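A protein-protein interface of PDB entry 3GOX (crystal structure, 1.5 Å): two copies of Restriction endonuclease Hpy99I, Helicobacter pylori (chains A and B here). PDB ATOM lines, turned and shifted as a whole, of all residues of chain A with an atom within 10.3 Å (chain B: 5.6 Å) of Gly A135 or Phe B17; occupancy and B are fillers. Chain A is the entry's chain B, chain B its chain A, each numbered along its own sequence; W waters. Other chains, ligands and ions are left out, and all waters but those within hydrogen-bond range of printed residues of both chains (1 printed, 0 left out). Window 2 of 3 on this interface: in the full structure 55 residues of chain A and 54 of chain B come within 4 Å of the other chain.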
ATOM      1  N   ALA A 131     -18.711   8.165   8.362  1.00  0.00           N
ATOM      2  CA  ALA A 131     -19.109   7.668   7.052  1.00  0.00           C
ATOM      3  C   ALA A 131     -19.658   6.247   7.138  1.00  0.00           C
ATOM      4  O   ALA A 131     -19.042   5.382   7.769  1.00  0.00           O
ATOM      5  CB  ALA A 131     -17.930   7.700   6.101  1.00  0.00           C
ATOM      6  N   PRO A 132     -20.813   5.985   6.500  1.00  0.00           N
ATOM      7  CA  PRO A 132     -21.290   4.600   6.388  1.00  0.00           C
ATOM      8  C   PRO A 132     -20.262   3.737   5.629  1.00  0.00           C
ATOM      9  O   PRO A 132     -19.820   4.140   4.552  1.00  0.00           O
ATOM     10  CB  PRO A 132     -22.590   4.742   5.580  1.00  0.00           C
ATOM     11  CG  PRO A 132     -22.997   6.167   5.730  1.00  0.00           C
ATOM     12  CD  PRO A 132     -21.738   6.949   5.873  1.00  0.00           C
ATOM     13  N   PRO A 133     -19.868   2.575   6.188  1.00  0.00           N
ATOM     14  CA  PRO A 133     -18.950   1.669   5.495  1.00  0.00           C
ATOM     15  C   PRO A 133     -19.476   1.202   4.143  1.00  0.00           C
ATOM     16  O   PRO A 133     -20.680   0.950   3.987  1.00  0.00           O
ATOM     17  CB  PRO A 133     -18.858   0.466   6.443  1.00  0.00           C
ATOM     18  CG  PRO A 133     -19.198   1.007   7.776  1.00  0.00           C
ATOM     19  CD  PRO A 133     -20.219   2.072   7.527  1.00  0.00           C
ATOM     20  N   LYS A 134     -18.581   1.079   3.163  1.00  0.00           N
ATOM     21  CA  LYS A 134     -18.933   0.489   1.879  1.00  0.00           C
ATOM     22  C   LYS A 134     -19.470  -0.908   2.172  1.00  0.00           C
ATOM     23  O   LYS A 134     -18.938  -1.626   2.999  1.00  0.00           O
ATOM     24  CB  LYS A 134     -17.711   0.393   0.952  1.00  0.00           C
ATOM     25  CG  LYS A 134     -18.066   0.283  -0.530  1.00  0.00           C
ATOM     26  CD  LYS A 134     -16.880  -0.246  -1.374  1.00  0.00           C
ATOM     27  CE  LYS A 134     -16.910   0.288  -2.803  1.00  0.00           C
ATOM     28  NZ  LYS A 134     -18.259   0.237  -3.441  1.00  0.00           N
ATOM     29  N   GLY A 135     -20.558  -1.282   1.516  1.00  0.00           N
ATOM     30  CA  GLY A 135     -21.131  -2.597   1.733  1.00  0.00           C
ATOM     31  C   GLY A 135     -22.014  -2.710   2.966  1.00  0.00           C
ATOM     32  O   GLY A 135     -22.480  -3.793   3.273  1.00  0.00           O
ATOM     33  N   SER A 136     -22.257  -1.625   3.686  1.00  0.00           N
ATOM     34  CA  SER A 136     -23.214  -1.660   4.801  1.00  0.00           C
ATOM     35  C   SER A 136     -24.635  -1.362   4.324  1.00  0.00           C
ATOM     36  O   SER A 136     -24.843  -0.841   3.242  1.00  0.00           O
ATOM     37  CB  SER A 136     -22.820  -0.689   5.912  1.00  0.00           C
ATOM     38  OG  SER A 136     -22.844   0.648   5.487  1.00  0.00           O
ATOM     39  N   VAL A 137     -25.613  -1.681   5.162  1.00  0.00           N
ATOM     40  CA  VAL A 137     -27.010  -1.379   4.857  1.00  0.00           C
ATOM     41  C   VAL A 137     -27.362   0.001   5.429  1.00  0.00           C
ATOM     42  O   VAL A 137     -27.246   0.233   6.641  1.00  0.00           O
ATOM     43  CB  VAL A 137     -27.944  -2.463   5.384  1.00  0.00           C
ATOM     44  CG1 VAL A 137     -29.403  -2.066   5.201  1.00  0.00           C
ATOM     45  CG2 VAL A 137     -27.687  -3.772   4.650  1.00  0.00           C
ATOM     46  N   PHE A 138     -27.756   0.908   4.537  1.00  0.00           N
ATOM     47  CA  PHE A 138     -27.938   2.323   4.825  1.00  0.00           C
ATOM     48  C   PHE A 138     -29.383   2.679   4.550  1.00  0.00           C
ATOM     49  O   PHE A 138     -30.008   2.096   3.677  1.00  0.00           O
ATOM     50  CB  PHE A 138     -27.047   3.126   3.870  1.00  0.00           C
ATOM     51  CG  PHE A 138     -27.176   4.632   3.972  1.00  0.00           C
ATOM     52  CD1 PHE A 138     -26.565   5.343   4.990  1.00  0.00           C
ATOM     53  CD2 PHE A 138     -27.845   5.335   2.985  1.00  0.00           C
ATOM     54  CE1 PHE A 138     -26.648   6.730   5.027  1.00  0.00           C
ATOM     55  CE2 PHE A 138     -27.944   6.701   3.026  1.00  0.00           C
ATOM     56  CZ  PHE A 138     -27.355   7.402   4.039  1.00  0.00           C
ATOM     57  N   ARG A 146     -33.844   2.194   1.611  1.00  0.00           N
ATOM     58  CA  ARG A 146     -32.759   1.348   2.093  1.00  0.00           C
ATOM     59  C   ARG A 146     -31.863   0.990   0.902  1.00  0.00           C
ATOM     60  O   ARG A 146     -32.330   0.881  -0.238  1.00  0.00           O
ATOM     61  CB  ARG A 146     -33.340   0.089   2.730  1.00  0.00           C
ATOM     62  CG  ARG A 146     -34.023   0.342   4.055  1.00  0.00           C
ATOM     63  CD  ARG A 146     -34.484  -0.939   4.710  1.00  0.00           C
ATOM     64  NE  ARG A 146     -35.532  -1.593   3.937  1.00  0.00           N
ATOM     65  CZ  ARG A 146     -36.810  -1.236   3.927  1.00  0.00           C
ATOM     66  NH1 ARG A 146     -37.239  -0.202   4.649  1.00  0.00           N
ATOM     67  NH2 ARG A 146     -37.665  -1.891   3.162  1.00  0.00           N
ATOM     68  N   SER A 147     -30.571   0.817   1.179  1.00  0.00           N
ATOM     69  CA  SER A 147     -29.603   0.461   0.149  1.00  0.00           C
ATOM     70  C   SER A 147     -28.395  -0.225   0.743  1.00  0.00           C
ATOM     71  O   SER A 147     -28.206  -0.209   1.970  1.00  0.00           O
ATOM     72  CB  SER A 147     -29.146   1.684  -0.643  1.00  0.00           C
ATOM     73  OG  SER A 147     -28.585   2.686   0.199  1.00  0.00           O
ATOM     74  N   ILE A 148     -27.602  -0.843  -0.123  1.00  0.00           N
ATOM     75  CA  ILE A 148     -26.310  -1.400   0.250  1.00  0.00           C
ATOM     76  C   ILE A 148     -25.292  -0.409  -0.289  1.00  0.00           C
ATOM     77  O   ILE A 148     -25.236  -0.175  -1.501  1.00  0.00           O
ATOM     78  CB  ILE A 148     -26.089  -2.782  -0.393  1.00  0.00           C
ATOM     79  CG1 ILE A 148     -27.158  -3.792   0.068  1.00  0.00           C
ATOM     80  CG2 ILE A 148     -24.680  -3.310  -0.065  1.00  0.00           C
ATOM     81  CD1 ILE A 148     -27.241  -5.074  -0.748  1.00  0.00           C
ATOM     82  N   VAL A 149     -24.497   0.196   0.595  1.00  0.00           N
ATOM     83  CA  VAL A 149     -23.626   1.334   0.222  1.00  0.00           C
ATOM     84  C   VAL A 149     -22.656   0.971  -0.891  1.00  0.00           C
ATOM     85  O   VAL A 149     -21.879   0.013  -0.772  1.00  0.00           O
ATOM     86  CB  VAL A 149     -22.827   1.862   1.413  1.00  0.00           C
ATOM     87  CG1 VAL A 149     -21.873   3.001   0.981  1.00  0.00           C
ATOM     88  CG2 VAL A 149     -23.782   2.347   2.512  1.00  0.00           C
ATOM     89  N   GLY A 150     -22.732   1.713  -1.991  1.00  0.00           N
ATOM     90  CA  GLY A 150     -21.845   1.512  -3.134  1.00  0.00           C
ATOM     91  C   GLY A 150     -22.195   0.335  -4.028  1.00  0.00           C
ATOM     92  O   GLY A 150     -21.442   0.026  -4.951  1.00  0.00           O
ATOM     93  N   VAL A 151     -23.334  -0.312  -3.761  1.00  0.00           N
ATOM     94  CA  VAL A 151     -23.836  -1.444  -4.546  1.00  0.00           C
ATOM     95  C   VAL A 151     -25.238  -1.157  -5.075  1.00  0.00           C
ATOM     96  O   VAL A 151     -25.467  -1.265  -6.275  1.00  0.00           O
ATOM     97  CB  VAL A 151     -23.789  -2.759  -3.728  1.00  0.00           C
ATOM     98  CG1 VAL A 151     -24.416  -3.898  -4.483  1.00  0.00           C
ATOM     99  CG2 VAL A 151     -22.344  -3.058  -3.379  1.00  0.00           C
ATOM    100  N   THR A 152     -26.173  -0.807  -4.201  1.00  0.00           N
ATOM    101  CA  THR A 152     -27.534  -0.444  -4.673  1.00  0.00           C
ATOM    102  C   THR A 152     -27.903   1.027  -4.512  1.00  0.00           C
ATOM    103  O   THR A 152     -28.992   1.447  -4.920  1.00  0.00           O
ATOM    104  CB  THR A 152     -28.652  -1.346  -4.080  1.00  0.00           C
ATOM    105  OG1 THR A 152     -28.724  -1.174  -2.647  1.00  0.00           O
ATOM    106  CG2 THR A 152     -28.426  -2.824  -4.416  1.00  0.00           C
ATOM    107  N   ALA A 153     -27.011   1.810  -3.926  1.00  0.00           N
ATOM    108  CA  ALA A 153     -27.046   3.266  -4.031  1.00  0.00           C
ATOM    109  C   ALA A 153     -25.678   3.810  -3.677  1.00  0.00           C
ATOM    110  O   ALA A 153     -25.002   3.270  -2.795  1.00  0.00           O
ATOM    111  CB  ALA A 153     -28.095   3.869  -3.116  1.00  0.00           C
ATOM    112  N   ASN A 154     -25.259   4.863  -4.367  1.00  0.00           N
ATOM    113  CA  ASN A 154     -24.037   5.587  -4.046  1.00  0.00           C
ATOM    114  C   ASN A 154     -24.363   6.774  -3.142  1.00  0.00           C
ATOM    115  O   ASN A 154     -25.364   7.477  -3.366  1.00  0.00           O
ATOM    116  CB  ASN A 154     -23.336   6.083  -5.314  1.00  0.00           C
ATOM    117  CG  ASN A 154     -22.804   4.946  -6.177  1.00  0.00           C
ATOM    118  OD1 ASN A 154     -22.516   3.852  -5.678  1.00  0.00           O
ATOM    119  ND2 ASN A 154     -22.644   5.207  -7.469  1.00  0.00           N
ATOM    120  N   LEU A 155     -23.508   7.001  -2.140  1.00  0.00           N
ATOM    121  CA  LEU A 155     -23.720   8.063  -1.155  1.00  0.00           C
ATOM    122  C   LEU A 155     -22.717   9.199  -1.343  1.00  0.00           C
ATOM    123  O   LEU A 155     -21.622   9.010  -1.896  1.00  0.00           O
ATOM    124  CB  LEU A 155     -23.600   7.526   0.288  1.00  0.00           C
ATOM    125  CG  LEU A 155     -24.425   6.313   0.718  1.00  0.00           C
ATOM    126  CD1 LEU A 155     -24.265   6.126   2.223  1.00  0.00           C
ATOM    127  CD2 LEU A 155     -25.902   6.435   0.324  1.00  0.00           C
ATOM    128  N   LEU B  12     -20.683 -18.478   8.129  1.00  0.00           N
ATOM    129  CA  LEU B  12     -21.268 -17.143   7.950  1.00  0.00           C
ATOM    130  C   LEU B  12     -20.815 -16.234   9.100  1.00  0.00           C
ATOM    131  O   LEU B  12     -20.643 -16.679  10.255  1.00  0.00           O
ATOM    132  CB  LEU B  12     -22.797 -17.186   7.848  1.00  0.00           C
ATOM    133  CG  LEU B  12     -23.385 -17.786   6.566  1.00  0.00           C
ATOM    134  CD1 LEU B  12     -24.887 -18.003   6.723  1.00  0.00           C
ATOM    135  CD2 LEU B  12     -23.115 -16.923   5.315  1.00  0.00           C
ATOM    136  N   ASP B  15     -22.452  -9.315   9.082  1.00  0.00           N
ATOM    137  CA  ASP B  15     -22.230  -8.346   8.000  1.00  0.00           C
ATOM    138  C   ASP B  15     -22.090  -9.010   6.633  1.00  0.00           C
ATOM    139  O   ASP B  15     -22.063  -8.302   5.624  1.00  0.00           O
ATOM    140  CB  ASP B  15     -21.062  -7.400   8.259  1.00  0.00           C
ATOM    141  CG  ASP B  15     -21.177  -6.680   9.586  1.00  0.00           C
ATOM    142  OD1 ASP B  15     -22.296  -6.333   9.987  1.00  0.00           O
ATOM    143  OD2 ASP B  15     -20.118  -6.401  10.184  1.00  0.00           O
ATOM    144  N   ASP B  16     -22.022 -10.341   6.584  1.00  0.00           N
ATOM    145  CA  ASP B  16     -22.011 -11.053   5.302  1.00  0.00           C
ATOM    146  C   ASP B  16     -23.368 -10.929   4.621  1.00  0.00           C
ATOM    147  O   ASP B  16     -24.405 -10.790   5.278  1.00  0.00           O
ATOM    148  CB  ASP B  16     -21.736 -12.552   5.456  1.00  0.00           C
ATOM    149  CG  ASP B  16     -20.301 -12.876   5.815  1.00  0.00           C
ATOM    150  OD1 ASP B  16     -19.402 -12.012   5.718  1.00  0.00           O
ATOM    151  OD2 ASP B  16     -20.089 -14.065   6.150  1.00  0.00           O
ATOM    152  N   PHE B  17     -23.355 -11.011   3.295  1.00  0.00           N
ATOM    153  CA  PHE B  17     -24.578 -11.020   2.493  1.00  0.00           C
ATOM    154  C   PHE B  17     -24.937 -12.406   1.974  1.00  0.00           C
ATOM    155  O   PHE B  17     -24.071 -13.199   1.623  1.00  0.00           O
ATOM    156  CB  PHE B  17     -24.445 -10.030   1.331  1.00  0.00           C
ATOM    157  CG  PHE B  17     -24.496  -8.599   1.774  1.00  0.00           C
ATOM    158  CD1 PHE B  17     -25.705  -7.962   1.972  1.00  0.00           C
ATOM    159  CD2 PHE B  17     -23.331  -7.910   2.046  1.00  0.00           C
ATOM    160  CE1 PHE B  17     -25.732  -6.647   2.416  1.00  0.00           C
ATOM    161  CE2 PHE B  17     -23.360  -6.599   2.486  1.00  0.00           C
ATOM    162  CZ  PHE B  17     -24.572  -5.976   2.668  1.00  0.00           C
ATOM    163  N   VAL B  18     -26.235 -12.691   1.968  1.00  0.00           N
ATOM    164  CA  VAL B  18     -26.763 -13.975   1.565  1.00  0.00           C
ATOM    165  C   VAL B  18     -28.014 -13.780   0.734  1.00  0.00           C
ATOM    166  O   VAL B  18     -28.639 -12.698   0.779  1.00  0.00           O
ATOM    167  CB  VAL B  18     -27.141 -14.839   2.788  1.00  0.00           C
ATOM    168  CG1 VAL B  18     -25.882 -15.225   3.564  1.00  0.00           C
ATOM    169  CG2 VAL B  18     -28.142 -14.121   3.696  1.00  0.00           C
ATOM    170  N   ILE B  19     -28.387 -14.829   0.011  1.00  0.00           N
ATOM    171  CA  ILE B  19     -29.726 -14.910  -0.548  1.00  0.00           C
ATOM    172  C   ILE B  19     -30.463 -16.076   0.089  1.00  0.00           C
ATOM    173  O   ILE B  19     -29.862 -17.085   0.484  1.00  0.00           O
ATOM    174  CB  ILE B  19     -29.740 -15.058  -2.088  1.00  0.00           C
ATOM    175  CG1 ILE B  19     -28.866 -16.229  -2.534  1.00  0.00           C
ATOM    176  CG2 ILE B  19     -29.328 -13.724  -2.733  1.00  0.00           C
ATOM    177  CD1 ILE B  19     -28.936 -16.500  -4.031  1.00  0.00           C
ATOM    178  N   VAL B  32     -32.141 -10.809  -0.995  1.00  0.00           N
ATOM    179  CA  VAL B  32     -30.854 -10.518  -0.364  1.00  0.00           C
ATOM    180  C   VAL B  32     -31.071 -10.099   1.079  1.00  0.00           C
ATOM    181  O   VAL B  32     -31.925  -9.272   1.402  1.00  0.00           O
ATOM    182  CB  VAL B  32     -30.081  -9.412  -1.120  1.00  0.00           C
ATOM    183  CG1 VAL B  32     -28.731  -9.091  -0.430  1.00  0.00           C
ATOM    184  CG2 VAL B  32     -29.855  -9.862  -2.557  1.00  0.00           C
ATOM    185  N   GLY B  33     -30.253 -10.674   1.950  1.00  0.00           N
ATOM    186  CA  GLY B  33     -30.218 -10.307   3.354  1.00  0.00           C
ATOM    187  C   GLY B  33     -28.801 -10.117   3.841  1.00  0.00           C
ATOM    188  O   GLY B  33     -27.841 -10.564   3.215  1.00  0.00           O
ATOM    189  N   VAL B  34     -28.688  -9.423   4.969  1.00  0.00           N
ATOM    190  CA  VAL B  34     -27.417  -9.248   5.672  1.00  0.00           C
ATOM    191  C   VAL B  34     -27.497  -9.985   7.025  1.00  0.00           C
ATOM    192  O   VAL B  34     -28.528  -9.965   7.730  1.00  0.00           O
ATOM    193  CB  VAL B  34     -27.074  -7.758   5.841  1.00  0.00           C
ATOM    194  CG1 VAL B  34     -28.123  -7.004   6.616  1.00  0.00           C
ATOM    195  CG2 VAL B  34     -25.697  -7.610   6.467  1.00  0.00           C
ATOM    196  N   ILE B  35     -26.411 -10.661   7.402  1.00  0.00           N
ATOM    197  CA  ILE B  35     -26.375 -11.404   8.656  1.00  0.00           C
ATOM    198  C   ILE B  35     -26.205 -10.437   9.821  1.00  0.00           C
ATOM    199  O   ILE B  35     -25.260  -9.648   9.829  1.00  0.00           O
ATOM    200  CB  ILE B  35     -25.210 -12.420   8.656  1.00  0.00           C
ATOM    201  CG1 ILE B  35     -25.329 -13.368   7.456  1.00  0.00           C
ATOM    202  CG2 ILE B  35     -25.131 -13.178   9.997  1.00  0.00           C
ATOM    203  CD1 ILE B  35     -26.597 -14.105   7.416  1.00  0.00           C
ATOM    204  N   ILE B  48     -33.549  -7.196   3.242  1.00  0.00           N
ATOM    205  CA  ILE B  48     -33.497  -5.744   3.093  1.00  0.00           C
ATOM    206  C   ILE B  48     -34.740  -5.173   2.399  1.00  0.00           C
ATOM    207  O   ILE B  48     -35.247  -4.122   2.808  1.00  0.00           O
ATOM    208  CB  ILE B  48     -32.216  -5.306   2.351  1.00  0.00           C
ATOM    209  CG1 ILE B  48     -30.989  -5.738   3.163  1.00  0.00           C
ATOM    210  CG2 ILE B  48     -32.219  -3.792   2.074  1.00  0.00           C
ATOM    211  CD1 ILE B  48     -29.714  -5.797   2.354  1.00  0.00           C
ATOM    212  N   GLU B  62     -27.469 -18.889   0.909  1.00  0.00           N
ATOM    213  CA  GLU B  62     -26.321 -18.986   0.034  1.00  0.00           C
ATOM    214  C   GLU B  62     -25.573 -17.639   0.095  1.00  0.00           C
ATOM    215  O   GLU B  62     -26.142 -16.587  -0.170  1.00  0.00           O
ATOM    216  CB  GLU B  62     -26.768 -19.286  -1.386  1.00  0.00           C
ATOM    217  CG  GLU B  62     -25.639 -19.435  -2.360  1.00  0.00           C
ATOM    218  CD  GLU B  62     -26.126 -19.728  -3.772  1.00  0.00           C
ATOM    219  OE1 GLU B  62     -27.238 -20.296  -3.941  1.00  0.00           O
ATOM    220  OE2 GLU B  62     -25.382 -19.390  -4.715  1.00  0.00           O
ATOM    221  N   ALA B  63     -24.296 -17.671   0.451  1.00  0.00           N
ATOM    222  CA  ALA B  63     -23.458 -16.473   0.454  1.00  0.00           C
ATOM    223  C   ALA B  63     -23.308 -15.936  -0.960  1.00  0.00           C
ATOM    224  O   ALA B  63     -23.164 -16.687  -1.921  1.00  0.00           O
ATOM    225  CB  ALA B  63     -22.066 -16.777   1.016  1.00  0.00           C
ATOM    226  N   ILE B  64     -23.365 -14.605  -1.064  1.00  0.00           N
ATOM    227  CA  ILE B  64     -23.091 -13.910  -2.315  1.00  0.00           C
ATOM    228  C   ILE B  64     -22.007 -12.843  -2.151  1.00  0.00           C
ATOM    229  O   ILE B  64     -21.758 -12.332  -1.042  1.00  0.00           O
ATOM    230  CB  ILE B  64     -24.373 -13.274  -2.919  1.00  0.00           C
ATOM    231  CG1 ILE B  64     -24.960 -12.184  -2.009  1.00  0.00           C
ATOM    232  CG2 ILE B  64     -25.393 -14.333  -3.197  1.00  0.00           C
ATOM    233  CD1 ILE B  64     -26.023 -11.279  -2.748  1.00  0.00           C
ATOM    234  N   ILE B  66     -21.432  -9.279  -3.189  1.00  0.00           N
ATOM    235  CA  ILE B  66     -22.135  -8.082  -3.679  1.00  0.00           C
ATOM    236  C   ILE B  66     -21.346  -7.336  -4.760  1.00  0.00           C
ATOM    237  O   ILE B  66     -21.940  -6.661  -5.604  1.00  0.00           O
ATOM    238  CB  ILE B  66     -22.532  -7.117  -2.524  1.00  0.00           C
ATOM    239  CG1 ILE B  66     -21.322  -6.633  -1.728  1.00  0.00           C
ATOM    240  CG2 ILE B  66     -23.616  -7.768  -1.663  1.00  0.00           C
ATOM    241  CD1 ILE B  66     -21.674  -5.675  -0.585  1.00  0.00           C
ATOM    242  N   TYR B  67     -20.022  -7.440  -4.729  1.00  0.00           N
ATOM    243  CA  TYR B  67     -19.177  -6.739  -5.698  1.00  0.00           C
ATOM    244  C   TYR B  67     -19.037  -7.444  -7.039  1.00  0.00           C
ATOM    245  O   TYR B  67     -18.404  -6.902  -7.961  1.00  0.00           O
ATOM    246  CB  TYR B  67     -17.817  -6.437  -5.084  1.00  0.00           C
ATOM    247  CG  TYR B  67     -17.946  -5.599  -3.830  1.00  0.00           C
ATOM    248  CD1 TYR B  67     -18.534  -4.341  -3.868  1.00  0.00           C
ATOM    249  CD2 TYR B  67     -17.547  -6.092  -2.602  1.00  0.00           C
ATOM    250  CE1 TYR B  67     -18.666  -3.576  -2.705  1.00  0.00           C
ATOM    251  CE2 TYR B  67     -17.673  -5.335  -1.452  1.00  0.00           C
ATOM    252  CZ  TYR B  67     -18.238  -4.095  -1.510  1.00  0.00           C
ATOM    253  OH  TYR B  67     -18.341  -3.391  -0.325  1.00  0.00           O
HETATM  254  O   HOH W   1     -22.538  -5.415   5.603  1.00  0.00           O
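O of Val B32 sits at hydrogen-bond distance from N of Ile B48, 3.2 Å away.
N of Ile A148 is in hydrogen-bond range of OG1 of Thr A152, 2.8 Å away.
N of Ile B64 lies within hydrogen-bond range of O of Phe B17, 3.1 Å away.
N of Gly A135 sits at hydrogen-bond distance from O of Val A149.
Of the printed residues of chain B, Gly A135 touches Phe B17 (3.0 Å), Ile B66 (3.9 Å) and Tyr B67 (3.6 Å).
Of chain A, only Gly A135 and Ile A148 come within 4 Å of Phe B17.
No residue of chain A comes within 4 Å of Asp B16.
No residue of chain A comes within 4 Å of Val B18.
Gly B33 touches none of the printed residues of chain A.
Ile B64 touches none of the printed residues of chain A.
Of the printed residues of chain B, Ile A148 touches Phe B17 (3.8 Å), Ile B48 (3.97 Å) and Ile B66 (3.9 Å).
Printed residues of chain A within 4 Å of Ile B66: Gly A135 (3.9 Å), Ile A148 (3.9 Å) and Val A151 (3.9 Å).
Of the printed residues of chain B, Lys A134 touches Tyr B67.
Of the printed residues of chain A, Ile B48 touches Val A137 (3.7 Å), Arg A146 (2.8 Å) and Ile A148 (3.97 Å).
Printed residues of chain A within 4 Å of Val B34: Val A137 (3.8 Å).
Glu B62 touches none of the printed residues of chain A.
Ser A147 touches none of the printed residues of chain B.
The nearest printed residue of chain B that does not touch Arg A146 is Val B32 (8.9 Å).
Lys A134 touches Tyr B67.
Gly A135 touches Phe B17.
Gly A135 touches Ile B66.
CA of Gly A135 touches OH of Tyr B67, 3.6 Å away.
Val B34 touches Val A137 (CG1 to CG2, 3.8 Å).
Ile B48 touches Val A137 (CD1 to CG2, 3.7 Å).
Ile A148 touches Phe B17.
Ile A148 touches Ile B48 (CG1 to CD1, 3.97 Å).
Ile A148 touches Ile B66 (CG2 to CD1, 3.9 Å).
CE1 of Tyr B67 touches CG2 of Val A151, 3.8 Å away.
No position is printed for both chains.
Of the 12 pairs that touch across the chains among the printed residues, none has its exchanged pair printed and touching as well.
NE of Arg A146 lies within hydrogen-bond range of O of Ile B48 (2.8 Å).
Of the 18 printed residues of chain A, 6 touch a printed residue of chain B.
Printed residues of chain B that touch a printed residue of chain A: Phe B17, Val B34, Ile B48, Ile B66 and Tyr B67.
Hydrophobic or aromatic side chains of chain B that line the printed part of chain A: Phe B17, Val B34, Ile B48, Ile B66 and Tyr B67.
Among the printed residues, 12 pairs touch across the chains.
Among the printed residues, no Asp or Glu carboxylate lies within 4 Å of a Lys or Arg side-chain nitrogen of the other chain.
Water W1 bridges the backbone carbonyl oxygen (O) of Gly A135 and the backbone carbonyl oxygen (O) of Asp B15.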
